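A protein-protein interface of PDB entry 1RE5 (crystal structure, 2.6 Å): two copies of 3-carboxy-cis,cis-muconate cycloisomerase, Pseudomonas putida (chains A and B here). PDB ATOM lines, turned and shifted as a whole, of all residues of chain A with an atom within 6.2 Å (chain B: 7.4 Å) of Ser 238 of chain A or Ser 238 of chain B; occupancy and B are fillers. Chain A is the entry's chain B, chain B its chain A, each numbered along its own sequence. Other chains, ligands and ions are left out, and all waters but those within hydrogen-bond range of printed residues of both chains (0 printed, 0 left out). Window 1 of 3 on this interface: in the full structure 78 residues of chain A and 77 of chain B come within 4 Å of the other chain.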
ATOM      1  N   LEU A 233     -17.003   3.976  -9.320  1.00  0.00           N
ATOM      2  CA  LEU A 233     -18.298   3.965  -8.654  1.00  0.00           C
ATOM      3  C   LEU A 233     -18.774   5.375  -8.340  1.00  0.00           C
ATOM      4  O   LEU A 233     -19.949   5.691  -8.517  1.00  0.00           O
ATOM      5  CB  LEU A 233     -18.226   3.136  -7.362  1.00  0.00           C
ATOM      6  CG  LEU A 233     -17.772   1.672  -7.477  1.00  0.00           C
ATOM      7  CD1 LEU A 233     -17.887   0.976  -6.122  1.00  0.00           C
ATOM      8  CD2 LEU A 233     -18.637   0.951  -8.501  1.00  0.00           C
ATOM      9  N   VAL A 234     -17.863   6.227  -7.884  1.00  0.00           N
ATOM     10  CA  VAL A 234     -18.228   7.583  -7.534  1.00  0.00           C
ATOM     11  C   VAL A 234     -18.656   8.353  -8.776  1.00  0.00           C
ATOM     12  O   VAL A 234     -19.573   9.180  -8.723  1.00  0.00           O
ATOM     13  CB  VAL A 234     -17.059   8.292  -6.810  1.00  0.00           C
ATOM     14  CG1 VAL A 234     -17.410   9.742  -6.502  1.00  0.00           C
ATOM     15  CG2 VAL A 234     -16.758   7.569  -5.514  1.00  0.00           C
ATOM     16  N   GLU A 235     -18.019   8.075  -9.908  1.00  0.00           N
ATOM     17  CA  GLU A 235     -18.396   8.772 -11.129  1.00  0.00           C
ATOM     18  C   GLU A 235     -19.845   8.430 -11.486  1.00  0.00           C
ATOM     19  O   GLU A 235     -20.651   9.319 -11.783  1.00  0.00           O
ATOM     20  CB  GLU A 235     -17.478   8.393 -12.289  1.00  0.00           C
ATOM     21  CG  GLU A 235     -18.053   8.794 -13.643  1.00  0.00           C
ATOM     22  CD  GLU A 235     -17.142   8.465 -14.810  1.00  0.00           C
ATOM     23  OE1 GLU A 235     -16.534   7.366 -14.818  1.00  0.00           O
ATOM     24  OE2 GLU A 235     -17.054   9.309 -15.731  1.00  0.00           O
ATOM     25  N   PHE A 236     -20.179   7.142 -11.455  1.00  0.00           N
ATOM     26  CA  PHE A 236     -21.538   6.715 -11.775  1.00  0.00           C
ATOM     27  C   PHE A 236     -22.558   7.402 -10.868  1.00  0.00           C
ATOM     28  O   PHE A 236     -23.602   7.863 -11.322  1.00  0.00           O
ATOM     29  CB  PHE A 236     -21.665   5.202 -11.616  1.00  0.00           C
ATOM     30  CG  PHE A 236     -23.050   4.682 -11.867  1.00  0.00           C
ATOM     31  CD1 PHE A 236     -23.627   4.781 -13.125  1.00  0.00           C
ATOM     32  CD2 PHE A 236     -23.769   4.073 -10.849  1.00  0.00           C
ATOM     33  CE1 PHE A 236     -24.899   4.274 -13.369  1.00  0.00           C
ATOM     34  CE2 PHE A 236     -25.045   3.562 -11.082  1.00  0.00           C
ATOM     35  CZ  PHE A 236     -25.606   3.662 -12.347  1.00  0.00           C
ATOM     36  N   ALA A 237     -22.252   7.457  -9.581  1.00  0.00           N
ATOM     37  CA  ALA A 237     -23.152   8.081  -8.620  1.00  0.00           C
ATOM     38  C   ALA A 237     -23.253   9.575  -8.919  1.00  0.00           C
ATOM     39  O   ALA A 237     -24.303  10.205  -8.745  1.00  0.00           O
ATOM     40  CB  ALA A 237     -22.627   7.855  -7.202  1.00  0.00           C
ATOM     41  N   SER A 238     -22.147  10.139  -9.379  1.00  0.00           N
ATOM     42  CA  SER A 238     -22.113  11.544  -9.702  1.00  0.00           C
ATOM     43  C   SER A 238     -23.035  11.917 -10.872  1.00  0.00           C
ATOM     44  O   SER A 238     -23.685  12.963 -10.841  1.00  0.00           O
ATOM     45  CB  SER A 238     -20.687  11.947 -10.016  1.00  0.00           C
ATOM     46  OG  SER A 238     -20.695  13.256 -10.534  1.00  0.00           O
ATOM     47  N   VAL A 239     -23.086  11.084 -11.908  1.00  0.00           N
ATOM     48  CA  VAL A 239     -23.956  11.375 -13.033  1.00  0.00           C
ATOM     49  C   VAL A 239     -25.404  11.199 -12.586  1.00  0.00           C
ATOM     50  O   VAL A 239     -26.287  11.988 -12.962  1.00  0.00           O
ATOM     51  CB  VAL A 239     -23.662  10.464 -14.240  1.00  0.00           C
ATOM     52  CG1 VAL A 239     -24.637  10.782 -15.383  1.00  0.00           C
ATOM     53  CG2 VAL A 239     -22.227  10.683 -14.708  1.00  0.00           C
ATOM     54  N   LEU A 240     -25.661  10.165 -11.793  1.00  0.00           N
ATOM     55  CA  LEU A 240     -27.007   9.978 -11.289  1.00  0.00           C
ATOM     56  C   LEU A 240     -27.377  11.241 -10.486  1.00  0.00           C
ATOM     57  O   LEU A 240     -28.546  11.638 -10.438  1.00  0.00           O
ATOM     58  CB  LEU A 240     -27.077   8.725 -10.408  1.00  0.00           C
ATOM     59  CG  LEU A 240     -27.676   7.474 -11.067  1.00  0.00           C
ATOM     60  CD1 LEU A 240     -27.076   7.279 -12.424  1.00  0.00           C
ATOM     61  CD2 LEU A 240     -27.414   6.252 -10.214  1.00  0.00           C
ATOM     62  N   GLY A 241     -26.369  11.870  -9.874  1.00  0.00           N
ATOM     63  CA  GLY A 241     -26.591  13.091  -9.115  1.00  0.00           C
ATOM     64  C   GLY A 241     -27.051  14.202 -10.043  1.00  0.00           C
ATOM     65  O   GLY A 241     -27.958  14.982  -9.733  1.00  0.00           O
ATOM     66  N   LEU A 242     -26.415  14.271 -11.202  1.00  0.00           N
ATOM     67  CA  LEU A 242     -26.755  15.261 -12.212  1.00  0.00           C
ATOM     68  C   LEU A 242     -28.202  15.073 -12.674  1.00  0.00           C
ATOM     69  O   LEU A 242     -28.937  16.044 -12.870  1.00  0.00           O
ATOM     70  CB  LEU A 242     -25.806  15.122 -13.404  1.00  0.00           C
ATOM     71  CG  LEU A 242     -24.650  16.106 -13.567  1.00  0.00           C
ATOM     72  CD1 LEU A 242     -24.173  16.630 -12.224  1.00  0.00           C
ATOM     73  CD2 LEU A 242     -23.541  15.408 -14.311  1.00  0.00           C
ATOM     74  N   VAL A 243     -28.609  13.819 -12.852  1.00  0.00           N
ATOM     75  CA  VAL A 243     -29.979  13.516 -13.262  1.00  0.00           C
ATOM     76  C   VAL A 243     -30.970  13.989 -12.181  1.00  0.00           C
ATOM     77  O   VAL A 243     -31.961  14.627 -12.489  1.00  0.00           O
ATOM     78  CB  VAL A 243     -30.167  11.977 -13.516  1.00  0.00           C
ATOM     79  CG1 VAL A 243     -31.628  11.638 -13.746  1.00  0.00           C
ATOM     80  CG2 VAL A 243     -29.367  11.552 -14.726  1.00  0.00           C
ATOM     81  N   LEU A 302     -24.232  11.522  -2.292  1.00  0.00           N
ATOM     82  CA  LEU A 302     -23.089  11.591  -3.192  1.00  0.00           C
ATOM     83  C   LEU A 302     -21.806  11.990  -2.496  1.00  0.00           C
ATOM     84  O   LEU A 302     -20.757  11.393  -2.731  1.00  0.00           O
ATOM     85  CB  LEU A 302     -23.312  12.622  -4.260  1.00  0.00           C
ATOM     86  CG  LEU A 302     -23.452  11.997  -5.605  1.00  0.00           C
ATOM     87  CD1 LEU A 302     -24.785  11.243  -5.665  1.00  0.00           C
ATOM     88  CD2 LEU A 302     -23.384  13.107  -6.627  1.00  0.00           C
ATOM     89  N   PHE A 306     -17.903  10.471  -2.242  1.00  0.00           N
ATOM     90  CA  PHE A 306     -16.651  11.199  -2.486  1.00  0.00           C
ATOM     91  C   PHE A 306     -15.807  11.076  -1.211  1.00  0.00           C
ATOM     92  O   PHE A 306     -14.618  10.758  -1.248  1.00  0.00           O
ATOM     93  CB  PHE A 306     -16.898  12.685  -2.781  1.00  0.00           C
ATOM     94  CG  PHE A 306     -17.185  12.976  -4.214  1.00  0.00           C
ATOM     95  CD1 PHE A 306     -18.491  13.140  -4.658  1.00  0.00           C
ATOM     96  CD2 PHE A 306     -16.155  13.044  -5.137  1.00  0.00           C
ATOM     97  CE1 PHE A 306     -18.771  13.370  -6.018  1.00  0.00           C
ATOM     98  CE2 PHE A 306     -16.423  13.271  -6.491  1.00  0.00           C
ATOM     99  CZ  PHE A 306     -17.740  13.434  -6.931  1.00  0.00           C
ATOM    100  N   ARG B 179     -11.698  11.678 -18.649  1.00  0.00           N
ATOM    101  CA  ARG B 179     -12.946  12.353 -18.305  1.00  0.00           C
ATOM    102  C   ARG B 179     -12.899  13.854 -18.636  1.00  0.00           C
ATOM    103  O   ARG B 179     -13.846  14.395 -19.211  1.00  0.00           O
ATOM    104  CB  ARG B 179     -13.248  12.141 -16.818  1.00  0.00           C
ATOM    105  CG  ARG B 179     -13.552  10.691 -16.455  1.00  0.00           C
ATOM    106  CD  ARG B 179     -13.639  10.468 -14.946  1.00  0.00           C
ATOM    107  NE  ARG B 179     -14.082   9.108 -14.643  1.00  0.00           N
ATOM    108  CZ  ARG B 179     -13.442   8.267 -13.830  1.00  0.00           C
ATOM    109  NH1 ARG B 179     -12.324   8.645 -13.220  1.00  0.00           N
ATOM    110  NH2 ARG B 179     -13.912   7.035 -13.643  1.00  0.00           N
ATOM    111  N   LEU B 183     -15.445  15.891 -21.278  1.00  0.00           N
ATOM    112  CA  LEU B 183     -16.326  16.986 -20.892  1.00  0.00           C
ATOM    113  C   LEU B 183     -15.965  18.327 -21.525  1.00  0.00           C
ATOM    114  O   LEU B 183     -16.800  19.236 -21.583  1.00  0.00           O
ATOM    115  CB  LEU B 183     -16.358  17.135 -19.363  1.00  0.00           C
ATOM    116  CG  LEU B 183     -15.147  17.681 -18.605  1.00  0.00           C
ATOM    117  CD1 LEU B 183     -15.075  19.189 -18.722  1.00  0.00           C
ATOM    118  CD2 LEU B 183     -15.269  17.295 -17.142  1.00  0.00           C
ATOM    119  N   ARG B 232     -23.569  21.402 -16.671  1.00  0.00           N
ATOM    120  CA  ARG B 232     -22.230  21.550 -17.203  1.00  0.00           C
ATOM    121  C   ARG B 232     -21.249  21.927 -16.118  1.00  0.00           C
ATOM    122  O   ARG B 232     -20.196  21.303 -15.993  1.00  0.00           O
ATOM    123  CB  ARG B 232     -22.204  22.572 -18.338  1.00  0.00           C
ATOM    124  CG  ARG B 232     -22.719  21.993 -19.640  1.00  0.00           C
ATOM    125  CD  ARG B 232     -22.688  22.992 -20.756  1.00  0.00           C
ATOM    126  NE  ARG B 232     -24.047  23.293 -21.171  1.00  0.00           N
ATOM    127  CZ  ARG B 232     -24.549  23.022 -22.366  1.00  0.00           C
ATOM    128  NH1 ARG B 232     -23.800  22.444 -23.296  1.00  0.00           N
ATOM    129  NH2 ARG B 232     -25.814  23.307 -22.610  1.00  0.00           N
ATOM    130  N   LEU B 233     -21.592  22.922 -15.309  1.00  0.00           N
ATOM    131  CA  LEU B 233     -20.688  23.337 -14.243  1.00  0.00           C
ATOM    132  C   LEU B 233     -20.539  22.269 -13.146  1.00  0.00           C
ATOM    133  O   LEU B 233     -19.441  22.004 -12.669  1.00  0.00           O
ATOM    134  CB  LEU B 233     -21.177  24.658 -13.635  1.00  0.00           C
ATOM    135  CG  LEU B 233     -21.307  25.856 -14.587  1.00  0.00           C
ATOM    136  CD1 LEU B 233     -21.838  27.091 -13.860  1.00  0.00           C
ATOM    137  CD2 LEU B 233     -19.947  26.138 -15.182  1.00  0.00           C
ATOM    138  N   VAL B 234     -21.642  21.646 -12.749  1.00  0.00           N
ATOM    139  CA  VAL B 234     -21.577  20.645 -11.697  1.00  0.00           C
ATOM    140  C   VAL B 234     -20.751  19.439 -12.139  1.00  0.00           C
ATOM    141  O   VAL B 234     -20.025  18.842 -11.338  1.00  0.00           O
ATOM    142  CB  VAL B 234     -22.981  20.192 -11.296  1.00  0.00           C
ATOM    143  CG1 VAL B 234     -22.899  19.141 -10.196  1.00  0.00           C
ATOM    144  CG2 VAL B 234     -23.789  21.396 -10.846  1.00  0.00           C
ATOM    145  N   GLU B 235     -20.852  19.082 -13.415  1.00  0.00           N
ATOM    146  CA  GLU B 235     -20.085  17.956 -13.913  1.00  0.00           C
ATOM    147  C   GLU B 235     -18.601  18.233 -13.750  1.00  0.00           C
ATOM    148  O   GLU B 235     -17.880  17.401 -13.209  1.00  0.00           O
ATOM    149  CB  GLU B 235     -20.398  17.678 -15.381  1.00  0.00           C
ATOM    150  CG  GLU B 235     -19.332  16.845 -16.040  1.00  0.00           C
ATOM    151  CD  GLU B 235     -19.690  16.418 -17.442  1.00  0.00           C
ATOM    152  OE1 GLU B 235     -20.120  17.274 -18.256  1.00  0.00           O
ATOM    153  OE2 GLU B 235     -19.523  15.209 -17.723  1.00  0.00           O
ATOM    154  N   PHE B 236     -18.147  19.397 -14.208  1.00  0.00           N
ATOM    155  CA  PHE B 236     -16.738  19.760 -14.090  1.00  0.00           C
ATOM    156  C   PHE B 236     -16.271  19.661 -12.637  1.00  0.00           C
ATOM    157  O   PHE B 236     -15.224  19.084 -12.332  1.00  0.00           O
ATOM    158  CB  PHE B 236     -16.533  21.184 -14.592  1.00  0.00           C
ATOM    159  CG  PHE B 236     -15.125  21.688 -14.448  1.00  0.00           C
ATOM    160  CD1 PHE B 236     -14.063  21.001 -15.001  1.00  0.00           C
ATOM    161  CD2 PHE B 236     -14.868  22.881 -13.791  1.00  0.00           C
ATOM    162  CE1 PHE B 236     -12.765  21.498 -14.902  1.00  0.00           C
ATOM    163  CE2 PHE B 236     -13.568  23.383 -13.693  1.00  0.00           C
ATOM    164  CZ  PHE B 236     -12.523  22.693 -14.247  1.00  0.00           C
ATOM    165  N   ALA B 237     -17.057  20.226 -11.734  1.00  0.00           N
ATOM    166  CA  ALA B 237     -16.711  20.206 -10.322  1.00  0.00           C
ATOM    167  C   ALA B 237     -16.624  18.758  -9.840  1.00  0.00           C
ATOM    168  O   ALA B 237     -15.769  18.399  -9.018  1.00  0.00           O
ATOM    169  CB  ALA B 237     -17.768  20.978  -9.519  1.00  0.00           C
ATOM    170  N   SER B 238     -17.517  17.926 -10.356  1.00  0.00           N
ATOM    171  CA  SER B 238     -17.528  16.543  -9.948  1.00  0.00           C
ATOM    172  C   SER B 238     -16.258  15.784 -10.351  1.00  0.00           C
ATOM    173  O   SER B 238     -15.790  14.915  -9.598  1.00  0.00           O
ATOM    174  CB  SER B 238     -18.747  15.840 -10.507  1.00  0.00           C
ATOM    175  OG  SER B 238     -18.586  14.454 -10.291  1.00  0.00           O
ATOM    176  N   VAL B 239     -15.703  16.086 -11.529  1.00  0.00           N
ATOM    177  CA  VAL B 239     -14.479  15.406 -11.950  1.00  0.00           C
ATOM    178  C   VAL B 239     -13.312  15.888 -11.079  1.00  0.00           C
ATOM    179  O   VAL B 239     -12.434  15.102 -10.701  1.00  0.00           O
ATOM    180  CB  VAL B 239     -14.144  15.652 -13.427  1.00  0.00           C
ATOM    181  CG1 VAL B 239     -12.844  14.937 -13.768  1.00  0.00           C
ATOM    182  CG2 VAL B 239     -15.263  15.124 -14.312  1.00  0.00           C
ATOM    183  N   LEU B 240     -13.304  17.181 -10.764  1.00  0.00           N
ATOM    184  CA  LEU B 240     -12.272  17.718  -9.902  1.00  0.00           C
ATOM    185  C   LEU B 240     -12.411  16.998  -8.555  1.00  0.00           C
ATOM    186  O   LEU B 240     -11.413  16.767  -7.858  1.00  0.00           O
ATOM    187  CB  LEU B 240     -12.469  19.221  -9.722  1.00  0.00           C
ATOM    188  CG  LEU B 240     -11.557  20.166 -10.514  1.00  0.00           C
ATOM    189  CD1 LEU B 240     -11.524  19.807 -11.975  1.00  0.00           C
ATOM    190  CD2 LEU B 240     -12.068  21.578 -10.345  1.00  0.00           C
ATOM    191  N   GLY B 241     -13.647  16.635  -8.197  1.00  0.00           N
ATOM    192  CA  GLY B 241     -13.892  15.938  -6.942  1.00  0.00           C
ATOM    193  C   GLY B 241     -13.230  14.574  -6.949  1.00  0.00           C
ATOM    194  O   GLY B 241     -12.637  14.134  -5.954  1.00  0.00           O
ATOM    195  N   LEU B 242     -13.351  13.891  -8.084  1.00  0.00           N
ATOM    196  CA  LEU B 242     -12.744  12.579  -8.278  1.00  0.00           C
ATOM    197  C   LEU B 242     -11.223  12.743  -8.138  1.00  0.00           C
ATOM    198  O   LEU B 242     -10.561  11.923  -7.498  1.00  0.00           O
ATOM    199  CB  LEU B 242     -13.088  12.056  -9.676  1.00  0.00           C
ATOM    200  CG  LEU B 242     -14.210  11.036  -9.908  1.00  0.00           C
ATOM    201  CD1 LEU B 242     -15.224  10.992  -8.770  1.00  0.00           C
ATOM    202  CD2 LEU B 242     -14.863  11.377 -11.218  1.00  0.00           C
ATOM    203  N   VAL B 243     -10.671  13.804  -8.723  1.00  0.00           N
ATOM    204  CA  VAL B 243      -9.237  14.053  -8.639  1.00  0.00           C
ATOM    205  C   VAL B 243      -8.779  14.236  -7.191  1.00  0.00           C
ATOM    206  O   VAL B 243      -7.783  13.636  -6.760  1.00  0.00           O
ATOM    207  CB  VAL B 243      -8.845  15.285  -9.459  1.00  0.00           C
ATOM    208  CG1 VAL B 243      -7.392  15.617  -9.231  1.00  0.00           C
ATOM    209  CG2 VAL B 243      -9.065  15.007 -10.934  1.00  0.00           C
ATOM    210  N   ALA B 244      -9.499  15.058  -6.434  1.00  0.00           N
ATOM    211  CA  ALA B 244      -9.161  15.290  -5.031  1.00  0.00           C
ATOM    212  C   ALA B 244      -9.193  13.963  -4.278  1.00  0.00           C
ATOM    213  O   ALA B 244      -8.311  13.681  -3.457  1.00  0.00           O
ATOM    214  CB  ALA B 244     -10.153  16.266  -4.410  1.00  0.00           C
ATOM    215  N   VAL B 298     -13.424  18.996  -0.233  1.00  0.00           N
ATOM    216  CA  VAL B 298     -14.133  19.004  -1.495  1.00  0.00           C
ATOM    217  C   VAL B 298     -15.512  18.346  -1.560  1.00  0.00           C
ATOM    218  O   VAL B 298     -16.410  18.877  -2.212  1.00  0.00           O
ATOM    219  CB  VAL B 298     -13.233  18.449  -2.605  1.00  0.00           C
ATOM    220  CG1 VAL B 298     -13.959  18.462  -3.929  1.00  0.00           C
ATOM    221  CG2 VAL B 298     -11.992  19.313  -2.720  1.00  0.00           C
ATOM    222  N   LEU B 302     -18.682  20.178  -3.252  1.00  0.00           N
ATOM    223  CA  LEU B 302     -19.309  19.570  -4.408  1.00  0.00           C
ATOM    224  C   LEU B 302     -20.795  19.371  -4.215  1.00  0.00           C
ATOM    225  O   LEU B 302     -21.568  19.626  -5.146  1.00  0.00           O
ATOM    226  CB  LEU B 302     -18.691  18.222  -4.703  1.00  0.00           C
ATOM    227  CG  LEU B 302     -18.002  18.246  -6.044  1.00  0.00           C
ATOM    228  CD1 LEU B 302     -16.803  19.167  -5.977  1.00  0.00           C
ATOM    229  CD2 LEU B 302     -17.594  16.825  -6.399  1.00  0.00           C
ATOM    230  N   LEU B 305     -22.832  22.369  -5.045  1.00  0.00           N
ATOM    231  CA  LEU B 305     -23.143  22.562  -6.447  1.00  0.00           C
ATOM    232  C   LEU B 305     -24.298  21.671  -6.877  1.00  0.00           C
ATOM    233  O   LEU B 305     -25.156  22.108  -7.631  1.00  0.00           O
ATOM    234  CB  LEU B 305     -21.893  22.334  -7.298  1.00  0.00           C
ATOM    235  CG  LEU B 305     -20.802  23.392  -7.036  1.00  0.00           C
ATOM    236  CD1 LEU B 305     -19.727  23.292  -8.112  1.00  0.00           C
ATOM    237  CD2 LEU B 305     -21.415  24.796  -7.056  1.00  0.00           C
ATOM    238  N   PHE B 306     -24.337  20.429  -6.403  1.00  0.00           N
ATOM    239  CA  PHE B 306     -25.457  19.554  -6.730  1.00  0.00           C
ATOM    240  C   PHE B 306     -26.735  20.153  -6.129  1.00  0.00           C
ATOM    241  O   PHE B 306     -27.765  20.267  -6.804  1.00  0.00           O
ATOM    242  CB  PHE B 306     -25.249  18.154  -6.168  1.00  0.00           C
ATOM    243  CG  PHE B 306     -24.393  17.273  -7.040  1.00  0.00           C
ATOM    244  CD1 PHE B 306     -23.066  17.018  -6.720  1.00  0.00           C
ATOM    245  CD2 PHE B 306     -24.905  16.736  -8.215  1.00  0.00           C
ATOM    246  CE1 PHE B 306     -22.270  16.251  -7.558  1.00  0.00           C
ATOM    247  CE2 PHE B 306     -24.105  15.968  -9.053  1.00  0.00           C
ATOM    248  CZ  PHE B 306     -22.786  15.729  -8.721  1.00  0.00           C
ATOM    249  N   MET B 309     -28.808  22.841  -8.059  1.00  0.00           N
ATOM    250  CA  MET B 309     -29.284  22.584  -9.411  1.00  0.00           C
ATOM    251  C   MET B 309     -30.735  22.883  -9.722  1.00  0.00           C
ATOM    252  O   MET B 309     -31.044  23.361 -10.808  1.00  0.00           O
ATOM    253  CB  MET B 309     -28.984  21.150  -9.814  1.00  0.00           C
ATOM    254  CG  MET B 309     -27.533  20.944 -10.180  1.00  0.00           C
ATOM    255  SD  MET B 309     -27.175  19.294 -10.789  1.00  0.00           S
ATOM    256  CE  MET B 309     -27.680  19.417 -12.526  1.00  0.00           C
ATOM    257  N   LEU B 327     -17.500  27.113  -6.767  1.00  0.00           N
ATOM    258  CA  LEU B 327     -16.730  26.510  -7.853  1.00  0.00           C
ATOM    259  C   LEU B 327     -15.276  26.944  -7.769  1.00  0.00           C
ATOM    260  O   LEU B 327     -14.361  26.122  -7.878  1.00  0.00           O
ATOM    261  CB  LEU B 327     -17.301  26.918  -9.205  1.00  0.00           C
ATOM    262  CG  LEU B 327     -17.404  25.842 -10.290  1.00  0.00           C
ATOM    263  CD1 LEU B 327     -17.865  26.497 -11.579  1.00  0.00           C
ATOM    264  CD2 LEU B 327     -16.086  25.149 -10.509  1.00  0.00           C
ATOM    265  N   ILE B 330     -13.295  25.084  -5.112  1.00  0.00           N
ATOM    266  CA  ILE B 330     -12.993  23.722  -5.530  1.00  0.00           C
ATOM    267  C   ILE B 330     -11.768  23.700  -6.432  1.00  0.00           C
ATOM    268  O   ILE B 330     -10.858  22.908  -6.218  1.00  0.00           O
ATOM    269  CB  ILE B 330     -14.193  23.101  -6.271  1.00  0.00           C
ATOM    270  CG1 ILE B 330     -15.379  22.990  -5.313  1.00  0.00           C
ATOM    271  CG2 ILE B 330     -13.826  21.737  -6.823  1.00  0.00           C
ATOM    272  CD1 ILE B 330     -16.639  22.571  -5.993  1.00  0.00           C
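Of chain B, only Ser 238 (2.4 Å) and Phe 306 (3.5 Å) come within 4 Å of Ser 238 of chain A. No residue of chain B comes within 4 Å of Ala 237 of chain A. Of the printed residues of chain A, Met 309 of chain B touches Leu 242 (3.6 Å). Of the printed residues of chain A, Leu 302 of chain B touches Phe 306. Printed residues of chain B within 4 Å of Phe 306 of chain A: Ser 238 (3.6 Å), Gly 241 (3.5 Å), Leu 242 (3.4 Å) and Leu 302 (3.4 Å). Of the printed residues of chain A, Arg 179 of chain B touches Glu 235. Ala 237 of chain B touches none of the printed residues of chain A. The nearest printed residue of chain B that does not touch Ser 238 of chain A is Glu 235 of chain B (5.7 Å). The nearest residue of chain A that does not touch Ser 238 of chain B is Val 234 of chain A (5.6 Å).
Among the printed residues, pairs that only touch across the chains: Val 234 of chain A with Leu 242 of chain B, Ser 238 of chain A with Phe 306 of chain B, Gly 241 of chain A with Phe 306 of chain B, Leu 242 of chain A with Val 234 of chain B, Leu 242 of chain A with Phe 306 of chain B, Leu 242 of chain A with Met 309 of chain B, Leu 302 of chain A with Phe 306 of chain B, Phe 306 of chain A with Ser 238 of chain B, Phe 306 of chain A with Gly 241 of chain B, Phe 306 of chain A with Leu 242 of chain B and Phe 306 of chain A with Leu 302 of chain B.
Of the 13 printed residues of chain A, 7 touch a printed residue of chain B. Hydrophobic or aromatic side chains of chain B within 4 Å of the printed part of chain A: Val 234, Leu 242, Leu 302, Phe 306 and Met 309.
The side-chain hydroxyl of Ser 238 of chain B sits at hydrogen-bond distance from the side-chain hydroxyl of Ser 238 of chain A (2.4 Å). The guanidinium group of Arg 179 of chain B is in salt-bridge range of the side-chain carboxylate of Glu 235 of chain A (2.9 Å).
Val 234 of chain A touches Leu 242 of chain B, and with the chains exchanged Leu 242 of chain A touches Val 234 of chain B. Ser 238 of chain A touches Phe 306 of chain B, and with the chains exchanged Phe 306 of chain A touches Ser 238 of chain B. Gly 241 of chain A touches Phe 306 of chain B, and with the chains exchanged Phe 306 of chain A touches Gly 241 of chain B. Leu 302 of chain A touches Phe 306 of chain B, and with the chains exchanged Phe 306 of chain A touches Leu 302 of chain B. Positions printed for both chains: 233, 234, 235, 236, 237, 238, 239, 240, 241, 242, 243, 302 and 306.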
